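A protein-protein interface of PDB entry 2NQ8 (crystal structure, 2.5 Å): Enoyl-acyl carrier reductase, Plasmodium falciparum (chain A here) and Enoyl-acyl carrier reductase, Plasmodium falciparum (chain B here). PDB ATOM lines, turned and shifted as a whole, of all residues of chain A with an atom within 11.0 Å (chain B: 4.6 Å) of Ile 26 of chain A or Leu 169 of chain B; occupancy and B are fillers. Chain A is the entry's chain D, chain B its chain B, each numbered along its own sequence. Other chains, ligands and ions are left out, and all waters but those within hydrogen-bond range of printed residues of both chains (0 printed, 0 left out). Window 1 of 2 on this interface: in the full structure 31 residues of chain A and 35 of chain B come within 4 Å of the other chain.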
ATOM      1  N   SER A  11      -1.408 -19.050 -24.578  1.00  0.00           N
ATOM      2  CA  SER A  11      -1.036 -17.817 -25.254  1.00  0.00           C
ATOM      3  C   SER A  11      -1.593 -17.780 -26.668  1.00  0.00           C
ATOM      4  O   SER A  11      -2.187 -16.791 -27.084  1.00  0.00           O
ATOM      5  CB  SER A  11       0.486 -17.669 -25.300  1.00  0.00           C
ATOM      6  OG  SER A  11       0.849 -16.449 -25.912  1.00  0.00           O
ATOM      7  N   GLN A  19      -0.865 -15.704 -34.106  1.00  0.00           N
ATOM      8  CA  GLN A  19       0.310 -16.399 -34.629  1.00  0.00           C
ATOM      9  C   GLN A  19       1.196 -17.040 -33.557  1.00  0.00           C
ATOM     10  O   GLN A  19       1.223 -16.600 -32.407  1.00  0.00           O
ATOM     11  CB  GLN A  19       1.159 -15.442 -35.471  1.00  0.00           C
ATOM     12  CG  GLN A  19       1.923 -14.388 -34.668  1.00  0.00           C
ATOM     13  CD  GLN A  19       1.527 -12.958 -35.028  1.00  0.00           C
ATOM     14  OE1 GLN A  19       2.279 -12.010 -34.776  1.00  0.00           O
ATOM     15  NE2 GLN A  19       0.338 -12.796 -35.611  1.00  0.00           N
ATOM     16  N   LYS A  20       1.914 -18.092 -33.943  1.00  0.00           N
ATOM     17  CA  LYS A  20       2.825 -18.760 -33.023  1.00  0.00           C
ATOM     18  C   LYS A  20       3.992 -17.808 -32.833  1.00  0.00           C
ATOM     19  O   LYS A  20       4.487 -17.228 -33.799  1.00  0.00           O
ATOM     20  CB  LYS A  20       3.338 -20.072 -33.617  1.00  0.00           C
ATOM     21  CG  LYS A  20       2.257 -21.113 -33.858  1.00  0.00           C
ATOM     22  CD  LYS A  20       2.796 -22.314 -34.633  1.00  0.00           C
ATOM     23  CE  LYS A  20       1.729 -23.386 -34.839  1.00  0.00           C
ATOM     24  NZ  LYS A  20       1.308 -24.025 -33.554  1.00  0.00           N
ATOM     25  N   LEU A  21       4.418 -17.642 -31.587  1.00  0.00           N
ATOM     26  CA  LEU A  21       5.534 -16.762 -31.257  1.00  0.00           C
ATOM     27  C   LEU A  21       6.821 -17.510 -31.554  1.00  0.00           C
ATOM     28  O   LEU A  21       7.016 -18.620 -31.073  1.00  0.00           O
ATOM     29  CB  LEU A  21       5.492 -16.382 -29.773  1.00  0.00           C
ATOM     30  CG  LEU A  21       6.535 -15.379 -29.278  1.00  0.00           C
ATOM     31  CD1 LEU A  21       6.247 -13.980 -29.863  1.00  0.00           C
ATOM     32  CD2 LEU A  21       6.517 -15.352 -27.757  1.00  0.00           C
ATOM     33  N   LEU A  22       7.697 -16.899 -32.341  1.00  0.00           N
ATOM     34  CA  LEU A  22       8.960 -17.530 -32.708  1.00  0.00           C
ATOM     35  C   LEU A  22      10.143 -16.831 -32.053  1.00  0.00           C
ATOM     36  O   LEU A  22      10.058 -15.651 -31.698  1.00  0.00           O
ATOM     37  CB  LEU A  22       9.137 -17.491 -34.228  1.00  0.00           C
ATOM     38  CG  LEU A  22       7.970 -17.985 -35.098  1.00  0.00           C
ATOM     39  CD1 LEU A  22       8.353 -17.857 -36.572  1.00  0.00           C
ATOM     40  CD2 LEU A  22       7.624 -19.433 -34.754  1.00  0.00           C
ATOM     41  N   SER A  23      11.242 -17.563 -31.893  1.00  0.00           N
ATOM     42  CA  SER A  23      12.444 -17.003 -31.302  1.00  0.00           C
ATOM     43  C   SER A  23      12.876 -15.782 -32.111  1.00  0.00           C
ATOM     44  O   SER A  23      13.316 -14.781 -31.544  1.00  0.00           O
ATOM     45  CB  SER A  23      13.568 -18.046 -31.292  1.00  0.00           C
ATOM     46  OG  SER A  23      13.750 -18.608 -32.582  1.00  0.00           O
ATOM     47  N   THR A  24      12.738 -15.863 -33.435  1.00  0.00           N
ATOM     48  CA  THR A  24      13.111 -14.750 -34.312  1.00  0.00           C
ATOM     49  C   THR A  24      12.262 -13.490 -34.096  1.00  0.00           C
ATOM     50  O   THR A  24      12.677 -12.391 -34.471  1.00  0.00           O
ATOM     51  CB  THR A  24      13.048 -15.158 -35.809  1.00  0.00           C
ATOM     52  OG1 THR A  24      11.791 -15.791 -36.091  1.00  0.00           O
ATOM     53  CG2 THR A  24      14.201 -16.110 -36.152  1.00  0.00           C
ATOM     54  N   ASP A  25      11.076 -13.649 -33.505  1.00  0.00           N
ATOM     55  CA  ASP A  25      10.217 -12.511 -33.215  1.00  0.00           C
ATOM     56  C   ASP A  25      10.876 -11.672 -32.105  1.00  0.00           C
ATOM     57  O   ASP A  25      10.914 -10.436 -32.174  1.00  0.00           O
ATOM     58  CB  ASP A  25       8.826 -12.981 -32.772  1.00  0.00           C
ATOM     59  CG  ASP A  25       8.001 -13.535 -33.925  1.00  0.00           C
ATOM     60  OD1 ASP A  25       8.133 -13.018 -35.054  1.00  0.00           O
ATOM     61  OD2 ASP A  25       7.209 -14.473 -33.705  1.00  0.00           O
ATOM     62  N   ILE A  26      11.390 -12.352 -31.082  1.00  0.00           N
ATOM     63  CA  ILE A  26      12.079 -11.674 -29.993  1.00  0.00           C
ATOM     64  C   ILE A  26      13.435 -11.239 -30.557  1.00  0.00           C
ATOM     65  O   ILE A  26      13.993 -10.202 -30.177  1.00  0.00           O
ATOM     66  CB  ILE A  26      12.292 -12.628 -28.781  1.00  0.00           C
ATOM     67  CG1 ILE A  26      10.996 -12.739 -27.959  1.00  0.00           C
ATOM     68  CG2 ILE A  26      13.470 -12.137 -27.923  1.00  0.00           C
ATOM     69  CD1 ILE A  26       9.819 -13.260 -28.728  1.00  0.00           C
ATOM     70  N   GLY A  27      13.947 -12.037 -31.488  1.00  0.00           N
ATOM     71  CA  GLY A  27      15.226 -11.741 -32.110  1.00  0.00           C
ATOM     72  C   GLY A  27      15.259 -10.423 -32.862  1.00  0.00           C
ATOM     73  O   GLY A  27      16.216  -9.662 -32.726  1.00  0.00           O
ATOM     74  N   SER A  28      14.219 -10.137 -33.643  1.00  0.00           N
ATOM     75  CA  SER A  28      14.181  -8.889 -34.406  1.00  0.00           C
ATOM     76  C   SER A  28      13.927  -7.654 -33.542  1.00  0.00           C
ATOM     77  O   SER A  28      14.322  -6.548 -33.906  1.00  0.00           O
ATOM     78  CB  SER A  28      13.129  -8.972 -35.506  1.00  0.00           C
ATOM     79  OG  SER A  28      11.872  -9.334 -34.971  1.00  0.00           O
ATOM     80  N   VAL A  29      13.258  -7.830 -32.407  1.00  0.00           N
ATOM     81  CA  VAL A  29      13.013  -6.710 -31.517  1.00  0.00           C
ATOM     82  C   VAL A  29      14.339  -6.436 -30.809  1.00  0.00           C
ATOM     83  O   VAL A  29      14.725  -5.280 -30.616  1.00  0.00           O
ATOM     84  CB  VAL A  29      11.920  -7.043 -30.480  1.00  0.00           C
ATOM     85  CG1 VAL A  29      11.704  -5.861 -29.530  1.00  0.00           C
ATOM     86  CG2 VAL A  29      10.626  -7.376 -31.197  1.00  0.00           C
ATOM     87  N   ALA A  30      15.043  -7.507 -30.444  1.00  0.00           N
ATOM     88  CA  ALA A  30      16.336  -7.386 -29.765  1.00  0.00           C
ATOM     89  C   ALA A  30      17.334  -6.721 -30.702  1.00  0.00           C
ATOM     90  O   ALA A  30      18.163  -5.907 -30.280  1.00  0.00           O
ATOM     91  CB  ALA A  30      16.856  -8.773 -29.347  1.00  0.00           C
ATOM     92  N   SER A  31      17.252  -7.078 -31.979  1.00  0.00           N
ATOM     93  CA  SER A  31      18.138  -6.506 -32.976  1.00  0.00           C
ATOM     94  C   SER A  31      17.901  -4.999 -33.017  1.00  0.00           C
ATOM     95  O   SER A  31      18.850  -4.213 -33.075  1.00  0.00           O
ATOM     96  CB  SER A  31      17.843  -7.119 -34.343  1.00  0.00           C
ATOM     97  OG  SER A  31      18.811  -6.714 -35.290  1.00  0.00           O
ATOM     98  N   PHE A  32      16.624  -4.611 -32.988  1.00  0.00           N
ATOM     99  CA  PHE A  32      16.220  -3.208 -33.008  1.00  0.00           C
ATOM    100  C   PHE A  32      16.735  -2.433 -31.783  1.00  0.00           C
ATOM    101  O   PHE A  32      17.351  -1.370 -31.913  1.00  0.00           O
ATOM    102  CB  PHE A  32      14.691  -3.119 -33.075  1.00  0.00           C
ATOM    103  CG  PHE A  32      14.148  -1.761 -32.739  1.00  0.00           C
ATOM    104  CD1 PHE A  32      14.349  -0.683 -33.597  1.00  0.00           C
ATOM    105  CD2 PHE A  32      13.484  -1.546 -31.531  1.00  0.00           C
ATOM    106  CE1 PHE A  32      13.902   0.592 -33.260  1.00  0.00           C
ATOM    107  CE2 PHE A  32      13.028  -0.271 -31.176  1.00  0.00           C
ATOM    108  CZ  PHE A  32      13.239   0.799 -32.041  1.00  0.00           C
ATOM    109  N   LEU A  33      16.471  -2.963 -30.595  1.00  0.00           N
ATOM    110  CA  LEU A  33      16.916  -2.323 -29.370  1.00  0.00           C
ATOM    111  C   LEU A  33      18.435  -2.177 -29.329  1.00  0.00           C
ATOM    112  O   LEU A  33      18.963  -1.256 -28.709  1.00  0.00           O
ATOM    113  CB  LEU A  33      16.444  -3.132 -28.161  1.00  0.00           C
ATOM    114  CG  LEU A  33      14.950  -3.046 -27.864  1.00  0.00           C
ATOM    115  CD1 LEU A  33      14.541  -4.150 -26.884  1.00  0.00           C
ATOM    116  CD2 LEU A  33      14.640  -1.661 -27.305  1.00  0.00           C
ATOM    117  N   LEU A  34      19.137  -3.095 -29.982  1.00  0.00           N
ATOM    118  CA  LEU A  34      20.593  -3.052 -30.011  1.00  0.00           C
ATOM    119  C   LEU A  34      21.128  -2.071 -31.042  1.00  0.00           C
ATOM    120  O   LEU A  34      22.243  -1.564 -30.905  1.00  0.00           O
ATOM    121  CB  LEU A  34      21.163  -4.450 -30.279  1.00  0.00           C
ATOM    122  CG  LEU A  34      21.012  -5.426 -29.109  1.00  0.00           C
ATOM    123  CD1 LEU A  34      21.504  -6.800 -29.525  1.00  0.00           C
ATOM    124  CD2 LEU A  34      21.802  -4.900 -27.897  1.00  0.00           C
ATOM    125  N   SER A  35      20.335  -1.798 -32.070  1.00  0.00           N
ATOM    126  CA  SER A  35      20.753  -0.867 -33.113  1.00  0.00           C
ATOM    127  C   SER A  35      20.516   0.595 -32.695  1.00  0.00           C
ATOM    128  O   SER A  35      19.773   0.874 -31.752  1.00  0.00           O
ATOM    129  CB  SER A  35      20.001  -1.158 -34.419  1.00  0.00           C
ATOM    130  OG  SER A  35      18.718  -0.548 -34.430  1.00  0.00           O
ATOM    131  N   GLN A  44      14.008   0.440 -20.190  1.00  0.00           N
ATOM    132  CA  GLN A  44      12.684  -0.113 -20.419  1.00  0.00           C
ATOM    133  C   GLN A  44      12.520  -1.634 -20.485  1.00  0.00           C
ATOM    134  O   GLN A  44      13.429  -2.380 -20.872  1.00  0.00           O
ATOM    135  CB  GLN A  44      12.122   0.462 -21.727  1.00  0.00           C
ATOM    136  CG  GLN A  44      12.140   1.975 -21.833  1.00  0.00           C
ATOM    137  CD  GLN A  44      11.199   2.604 -20.857  1.00  0.00           C
ATOM    138  OE1 GLN A  44       9.985   2.496 -21.002  1.00  0.00           O
ATOM    139  NE2 GLN A  44      11.749   3.251 -19.835  1.00  0.00           N
ATOM    140  N   THR A  45      11.317  -2.062 -20.116  1.00  0.00           N
ATOM    141  CA  THR A  45      10.903  -3.448 -20.181  1.00  0.00           C
ATOM    142  C   THR A  45       9.985  -3.445 -21.402  1.00  0.00           C
ATOM    143  O   THR A  45       8.867  -2.936 -21.342  1.00  0.00           O
ATOM    144  CB  THR A  45      10.057  -3.870 -18.972  1.00  0.00           C
ATOM    145  OG1 THR A  45      10.861  -3.890 -17.788  1.00  0.00           O
ATOM    146  CG2 THR A  45       9.479  -5.255 -19.205  1.00  0.00           C
ATOM    147  N   ILE A  46      10.462  -3.983 -22.516  1.00  0.00           N
ATOM    148  CA  ILE A  46       9.648  -4.022 -23.716  1.00  0.00           C
ATOM    149  C   ILE A  46       9.053  -5.403 -23.938  1.00  0.00           C
ATOM    150  O   ILE A  46       9.767  -6.398 -24.064  1.00  0.00           O
ATOM    151  CB  ILE A  46      10.459  -3.602 -24.961  1.00  0.00           C
ATOM    152  CG1 ILE A  46      10.643  -2.086 -24.963  1.00  0.00           C
ATOM    153  CG2 ILE A  46       9.753  -4.053 -26.225  1.00  0.00           C
ATOM    154  CD1 ILE A  46      11.593  -1.613 -23.924  1.00  0.00           C
ATOM    155  N   TYR A  47       7.731  -5.445 -23.984  1.00  0.00           N
ATOM    156  CA  TYR A  47       7.005  -6.684 -24.186  1.00  0.00           C
ATOM    157  C   TYR A  47       6.928  -7.114 -25.642  1.00  0.00           C
ATOM    158  O   TYR A  47       6.624  -6.309 -26.535  1.00  0.00           O
ATOM    159  CB  TYR A  47       5.590  -6.551 -23.625  1.00  0.00           C
ATOM    160  CG  TYR A  47       5.526  -6.699 -22.122  1.00  0.00           C
ATOM    161  CD1 TYR A  47       5.315  -7.951 -21.532  1.00  0.00           C
ATOM    162  CD2 TYR A  47       5.656  -5.583 -21.284  1.00  0.00           C
ATOM    163  CE1 TYR A  47       5.228  -8.078 -20.135  1.00  0.00           C
ATOM    164  CE2 TYR A  47       5.570  -5.702 -19.899  1.00  0.00           C
ATOM    165  CZ  TYR A  47       5.354  -6.944 -19.335  1.00  0.00           C
ATOM    166  OH  TYR A  47       5.237  -7.050 -17.972  1.00  0.00           O
ATOM    167  N   VAL A  48       7.214  -8.397 -25.861  1.00  0.00           N
ATOM    168  CA  VAL A  48       7.173  -9.017 -27.178  1.00  0.00           C
ATOM    169  C   VAL A  48       6.589 -10.396 -26.876  1.00  0.00           C
ATOM    170  O   VAL A  48       7.308 -11.394 -26.742  1.00  0.00           O
ATOM    171  CB  VAL A  48       8.593  -9.124 -27.789  1.00  0.00           C
ATOM    172  CG1 VAL A  48       8.515  -9.665 -29.208  1.00  0.00           C
ATOM    173  CG2 VAL A  48       9.264  -7.742 -27.794  1.00  0.00           C
ATOM    174  N   ASP A  49       5.262 -10.421 -26.775  1.00  0.00           N
ATOM    175  CA  ASP A  49       4.508 -11.611 -26.406  1.00  0.00           C
ATOM    176  C   ASP A  49       3.120 -11.598 -27.040  1.00  0.00           C
ATOM    177  O   ASP A  49       2.150 -12.046 -26.422  1.00  0.00           O
ATOM    178  CB  ASP A  49       4.329 -11.603 -24.894  1.00  0.00           C
ATOM    179  CG  ASP A  49       3.489 -10.416 -24.430  1.00  0.00           C
ATOM    180  OD1 ASP A  49       3.304  -9.472 -25.231  1.00  0.00           O
ATOM    181  OD2 ASP A  49       3.014 -10.420 -23.276  1.00  0.00           O
ATOM    182  N   ASN A  50       3.019 -11.070 -28.251  1.00  0.00           N
ATOM    183  CA  ASN A  50       1.740 -10.997 -28.958  1.00  0.00           C
ATOM    184  C   ASN A  50       0.628 -10.298 -28.169  1.00  0.00           C
ATOM    185  O   ASN A  50      -0.562 -10.554 -28.388  1.00  0.00           O
ATOM    186  CB  ASN A  50       1.278 -12.400 -29.374  1.00  0.00           C
ATOM    187  CG  ASN A  50       2.200 -13.036 -30.405  1.00  0.00           C
ATOM    188  OD1 ASN A  50       2.669 -12.362 -31.330  1.00  0.00           O
ATOM    189  ND2 ASN A  50       2.454 -14.338 -30.260  1.00  0.00           N
ATOM    190  N   GLY A  51       1.029  -9.427 -27.241  1.00  0.00           N
ATOM    191  CA  GLY A  51       0.075  -8.665 -26.448  1.00  0.00           C
ATOM    192  C   GLY A  51      -0.626  -9.339 -25.275  1.00  0.00           C
ATOM    193  O   GLY A  51      -1.509  -8.719 -24.679  1.00  0.00           O
ATOM    194  N   TYR B  15      16.143 -18.445 -27.016  1.00  0.00           N
ATOM    195  CA  TYR B  15      15.989 -17.107 -27.590  1.00  0.00           C
ATOM    196  C   TYR B  15      17.305 -16.557 -28.119  1.00  0.00           C
ATOM    197  O   TYR B  15      17.321 -15.798 -29.086  1.00  0.00           O
ATOM    198  CB  TYR B  15      15.388 -16.141 -26.561  1.00  0.00           C
ATOM    199  CG  TYR B  15      13.875 -16.205 -26.487  1.00  0.00           C
ATOM    200  CD1 TYR B  15      13.105 -16.052 -27.638  1.00  0.00           C
ATOM    201  CD2 TYR B  15      13.209 -16.414 -25.268  1.00  0.00           C
ATOM    202  CE1 TYR B  15      11.710 -16.104 -27.597  1.00  0.00           C
ATOM    203  CE2 TYR B  15      11.803 -16.469 -25.212  1.00  0.00           C
ATOM    204  CZ  TYR B  15      11.065 -16.310 -26.389  1.00  0.00           C
ATOM    205  OH  TYR B  15       9.686 -16.334 -26.376  1.00  0.00           O
ATOM    206  N   ILE B  19      18.065 -14.631 -31.536  1.00  0.00           N
ATOM    207  CA  ILE B  19      18.638 -13.292 -31.506  1.00  0.00           C
ATOM    208  C   ILE B  19      19.882 -13.233 -32.388  1.00  0.00           C
ATOM    209  O   ILE B  19      20.090 -12.257 -33.118  1.00  0.00           O
ATOM    210  CB  ILE B  19      19.013 -12.873 -30.058  1.00  0.00           C
ATOM    211  CG1 ILE B  19      17.734 -12.690 -29.232  1.00  0.00           C
ATOM    212  CG2 ILE B  19      19.835 -11.588 -30.072  1.00  0.00           C
ATOM    213  CD1 ILE B  19      17.983 -12.315 -27.780  1.00  0.00           C
ATOM    214  N   HIS B 118      22.246 -10.504 -22.788  1.00  0.00           N
ATOM    215  CA  HIS B 118      22.118 -11.401 -21.643  1.00  0.00           C
ATOM    216  C   HIS B 118      20.869 -12.252 -21.902  1.00  0.00           C
ATOM    217  O   HIS B 118      19.735 -11.764 -21.844  1.00  0.00           O
ATOM    218  CB  HIS B 118      21.982 -10.593 -20.354  1.00  0.00           C
ATOM    219  CG  HIS B 118      21.844 -11.425 -19.117  1.00  0.00           C
ATOM    220  ND1 HIS B 118      20.687 -12.106 -18.802  1.00  0.00           N
ATOM    221  CD2 HIS B 118      22.685 -11.611 -18.070  1.00  0.00           C
ATOM    222  CE1 HIS B 118      20.818 -12.668 -17.611  1.00  0.00           C
ATOM    223  NE2 HIS B 118      22.020 -12.382 -17.145  1.00  0.00           N
ATOM    224  N   SER B 119      21.096 -13.521 -22.221  1.00  0.00           N
ATOM    225  CA  SER B 119      20.012 -14.437 -22.523  1.00  0.00           C
ATOM    226  C   SER B 119      20.081 -15.685 -21.662  1.00  0.00           C
ATOM    227  O   SER B 119      20.040 -16.807 -22.172  1.00  0.00           O
ATOM    228  CB  SER B 119      20.071 -14.834 -24.003  1.00  0.00           C
ATOM    229  OG  SER B 119      18.983 -15.676 -24.338  1.00  0.00           O
ATOM    230  N   SER B 168      18.578  -7.805 -22.160  1.00  0.00           N
ATOM    231  CA  SER B 168      18.431  -9.066 -21.446  1.00  0.00           C
ATOM    232  C   SER B 168      16.975  -9.496 -21.632  1.00  0.00           C
ATOM    233  O   SER B 168      16.190  -8.744 -22.207  1.00  0.00           O
ATOM    234  CB  SER B 168      18.767  -8.892 -19.960  1.00  0.00           C
ATOM    235  OG  SER B 168      17.851  -8.030 -19.309  1.00  0.00           O
ATOM    236  N   LEU B 169      16.626 -10.699 -21.176  1.00  0.00           N
ATOM    237  CA  LEU B 169      15.256 -11.203 -21.301  1.00  0.00           C
ATOM    238  C   LEU B 169      14.586 -11.366 -19.937  1.00  0.00           C
ATOM    239  O   LEU B 169      15.228 -11.718 -18.947  1.00  0.00           O
ATOM    240  CB  LEU B 169      15.227 -12.557 -22.031  1.00  0.00           C
ATOM    241  CG  LEU B 169      15.552 -12.638 -23.528  1.00  0.00           C
ATOM    242  CD1 LEU B 169      14.583 -11.768 -24.310  1.00  0.00           C
ATOM    243  CD2 LEU B 169      16.970 -12.182 -23.777  1.00  0.00           C
ATOM    244  N   THR B 170      13.285 -11.121 -19.895  1.00  0.00           N
ATOM    245  CA  THR B 170      12.529 -11.250 -18.655  1.00  0.00           C
ATOM    246  C   THR B 170      11.164 -11.838 -18.956  1.00  0.00           C
ATOM    247  O   THR B 170      10.823 -12.064 -20.110  1.00  0.00           O
ATOM    248  CB  THR B 170      12.332  -9.883 -17.960  1.00  0.00           C
ATOM    249  OG1 THR B 170      11.583 -10.071 -16.752  1.00  0.00           O
ATOM    250  CG2 THR B 170      11.587  -8.907 -18.890  1.00  0.00           C
ATOM    251  N   LYS B 189      13.356 -12.145 -11.823  1.00  0.00           N
ATOM    252  CA  LYS B 189      12.924 -11.328 -12.943  1.00  0.00           C
ATOM    253  C   LYS B 189      12.543  -9.927 -12.461  1.00  0.00           C
ATOM    254  O   LYS B 189      12.844  -8.939 -13.131  1.00  0.00           O
ATOM    255  CB  LYS B 189      11.748 -11.991 -13.664  1.00  0.00           C
ATOM    256  CG  LYS B 189      12.122 -13.291 -14.362  1.00  0.00           C
ATOM    257  CD  LYS B 189      13.315 -13.080 -15.284  1.00  0.00           C
ATOM    258  CE  LYS B 189      13.618 -14.313 -16.101  1.00  0.00           C
ATOM    259  NZ  LYS B 189      14.847 -14.166 -16.939  1.00  0.00           N
ATOM    260  N   LEU B 192      15.785  -8.063 -11.929  1.00  0.00           N
ATOM    261  CA  LEU B 192      16.397  -7.773 -13.222  1.00  0.00           C
ATOM    262  C   LEU B 192      15.752  -6.516 -13.844  1.00  0.00           C
ATOM    263  O   LEU B 192      16.443  -5.622 -14.344  1.00  0.00           O
ATOM    264  CB  LEU B 192      16.214  -8.984 -14.151  1.00  0.00           C
ATOM    265  CG  LEU B 192      16.837  -8.993 -15.553  1.00  0.00           C
ATOM    266  CD1 LEU B 192      18.333  -9.189 -15.435  1.00  0.00           C
ATOM    267  CD2 LEU B 192      16.246 -10.128 -16.375  1.00  0.00           C
ATOM    268  N   THR B 213      15.300  -4.323 -21.426  1.00  0.00           N
ATOM    269  CA  THR B 213      15.002  -5.730 -21.245  1.00  0.00           C
ATOM    270  C   THR B 213      13.756  -6.133 -22.043  1.00  0.00           C
ATOM    271  O   THR B 213      12.860  -5.322 -22.269  1.00  0.00           O
ATOM    272  CB  THR B 213      14.814  -6.053 -19.761  1.00  0.00           C
ATOM    273  OG1 THR B 213      14.595  -7.463 -19.614  1.00  0.00           O
ATOM    274  CG2 THR B 213      13.643  -5.262 -19.187  1.00  0.00           C
ATOM    275  N   ILE B 214      13.710  -7.388 -22.476  1.00  0.00           N
ATOM    276  CA  ILE B 214      12.577  -7.885 -23.251  1.00  0.00           C
ATOM    277  C   ILE B 214      11.771  -8.947 -22.497  1.00  0.00           C
ATOM    278  O   ILE B 214      12.304  -9.994 -22.125  1.00  0.00           O
ATOM    279  CB  ILE B 214      13.047  -8.482 -24.598  1.00  0.00           C
ATOM    280  CG1 ILE B 214      13.532  -7.361 -25.521  1.00  0.00           C
ATOM    281  CG2 ILE B 214      11.906  -9.277 -25.254  1.00  0.00           C
ATOM    282  CD1 ILE B 214      14.126  -7.856 -26.849  1.00  0.00           C
ATOM    283  N   ALA B 216       9.471 -11.662 -22.817  1.00  0.00           N
ATOM    284  CA  ALA B 216       9.044 -12.588 -23.863  1.00  0.00           C
ATOM    285  C   ALA B 216       7.879 -13.509 -23.569  1.00  0.00           C
ATOM    286  O   ALA B 216       7.594 -13.832 -22.409  1.00  0.00           O
ATOM    287  CB  ALA B 216      10.227 -13.426 -24.300  1.00  0.00           C
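Among the printed residues, merely in contact across the chains: Ile 46 of chain A with Ile 214 of chain B, Thr 45 of chain A with Thr 213 of chain B, Ile 26 of chain A with Tyr 15 of chain B, Val 48 of chain A with Ala 216 of chain B, Leu 21 of chain A with Tyr 15 of chain B, Leu 33 of chain A with Ile 214 of chain B, Ala 30 of chain A with Ile 214 of chain B, Gly 27 of chain A with Ile 19 of chain B, Ile 26 of chain A with Leu 169 of chain B, Ile 26 of chain A with Ala 216 of chain B, Ser 23 of chain A with Tyr 15 of chain B and Val 48 of chain A with Ile 214 of chain B.
Hydrophobic or aromatic side chains of chain B that line the printed part of chain A: Tyr 15, Ile 19, Leu 169, Ile 214 and Ala 216.
Among the printed residues, 14 pairs touch across the chains.
Among the printed residues, no Asp or Glu carboxylate lies within 4 Å of a Lys or Arg side-chain nitrogen of the other chain.
Printed residues of chain B within 4 Å of Ser 23 of chain A: Tyr 15 (3.8 Å).
Of chain B, only Tyr 15 (3.5 Å), Leu 169 (3.8 Å) and Ala 216 (3.8 Å) come within 4 Å of Ile 26 of chain A.
Of the printed residues of chain B, Gly 27 of chain A touches Ile 19.
Ser 35 of chain A touches none of the printed residues of chain B.
Of the printed residues of chain B, Thr 45 of chain A touches Thr 213 (3.4 Å).
Of the printed residues of chain B, Ile 46 of chain A touches Thr 213 (2.8 Å) and Ile 214 (3.3 Å).
Of the printed residues of chain B, Val 48 of chain A touches Ile 214 and Ala 216.
No residue of chain A comes within 4 Å of His 118 of chain B.
No residue of chain A comes within 4 Å of Ser 119 of chain B.
No residue of chain A comes within 4 Å of Ser 168 of chain B.
Of chain A, only Ile 26 (3.8 Å) comes within 4 Å of Leu 169 of chain B.
No residue of chain A comes within 4 Å of Thr 170 of chain B.
Of the printed residues of chain A, Thr 213 of chain B touches Gln 44 (2.8 Å), Thr 45 (3.4 Å) and Ile 46 (2.8 Å).
Ala 216 of chain B touches just these residues of chain A: Ile 26 and Val 48.
The nearest residue of chain A that does not touch Leu 169 of chain B is Ala 30 of chain A (6.3 Å).
The nearest printed residue of chain B that does not touch Leu 21 of chain A is Ala 216 of chain B (4.8 Å).
The backbone NH (N) of Thr 213 of chain B lies within hydrogen-bond range of the backbone carbonyl oxygen (O) of Gln 44 of chain A (2.8 Å).
The backbone NH (N) of Ile 46 of chain A lies within hydrogen-bond range of the backbone carbonyl oxygen (O) of Thr 213 of chain B (2.8 Å).
N of Leu 169 of chain B sits at hydrogen-bond distance from O of His 118 of chain B (3.4 Å).
O of Ser 168 of chain B lies within hydrogen-bond range of OG1 of Thr 213 of chain B (3.3 Å).
The backbone carbonyl oxygen of Ser 168 of chain B lies within hydrogen-bond range of the backbone NH of Ile 214 of chain B.
NZ of Lys 189 of chain B sits at hydrogen-bond distance from O of Leu 169 of chain B, 3.2 Å away.
The backbone NH of Thr 170 of chain B lies within hydrogen-bond range of the backbone carbonyl oxygen of Ile 214 of chain B, 2.7 Å away.
O of Thr 170 of chain B sits at hydrogen-bond distance from N of Ala 216 of chain B, 3.1 Å away.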
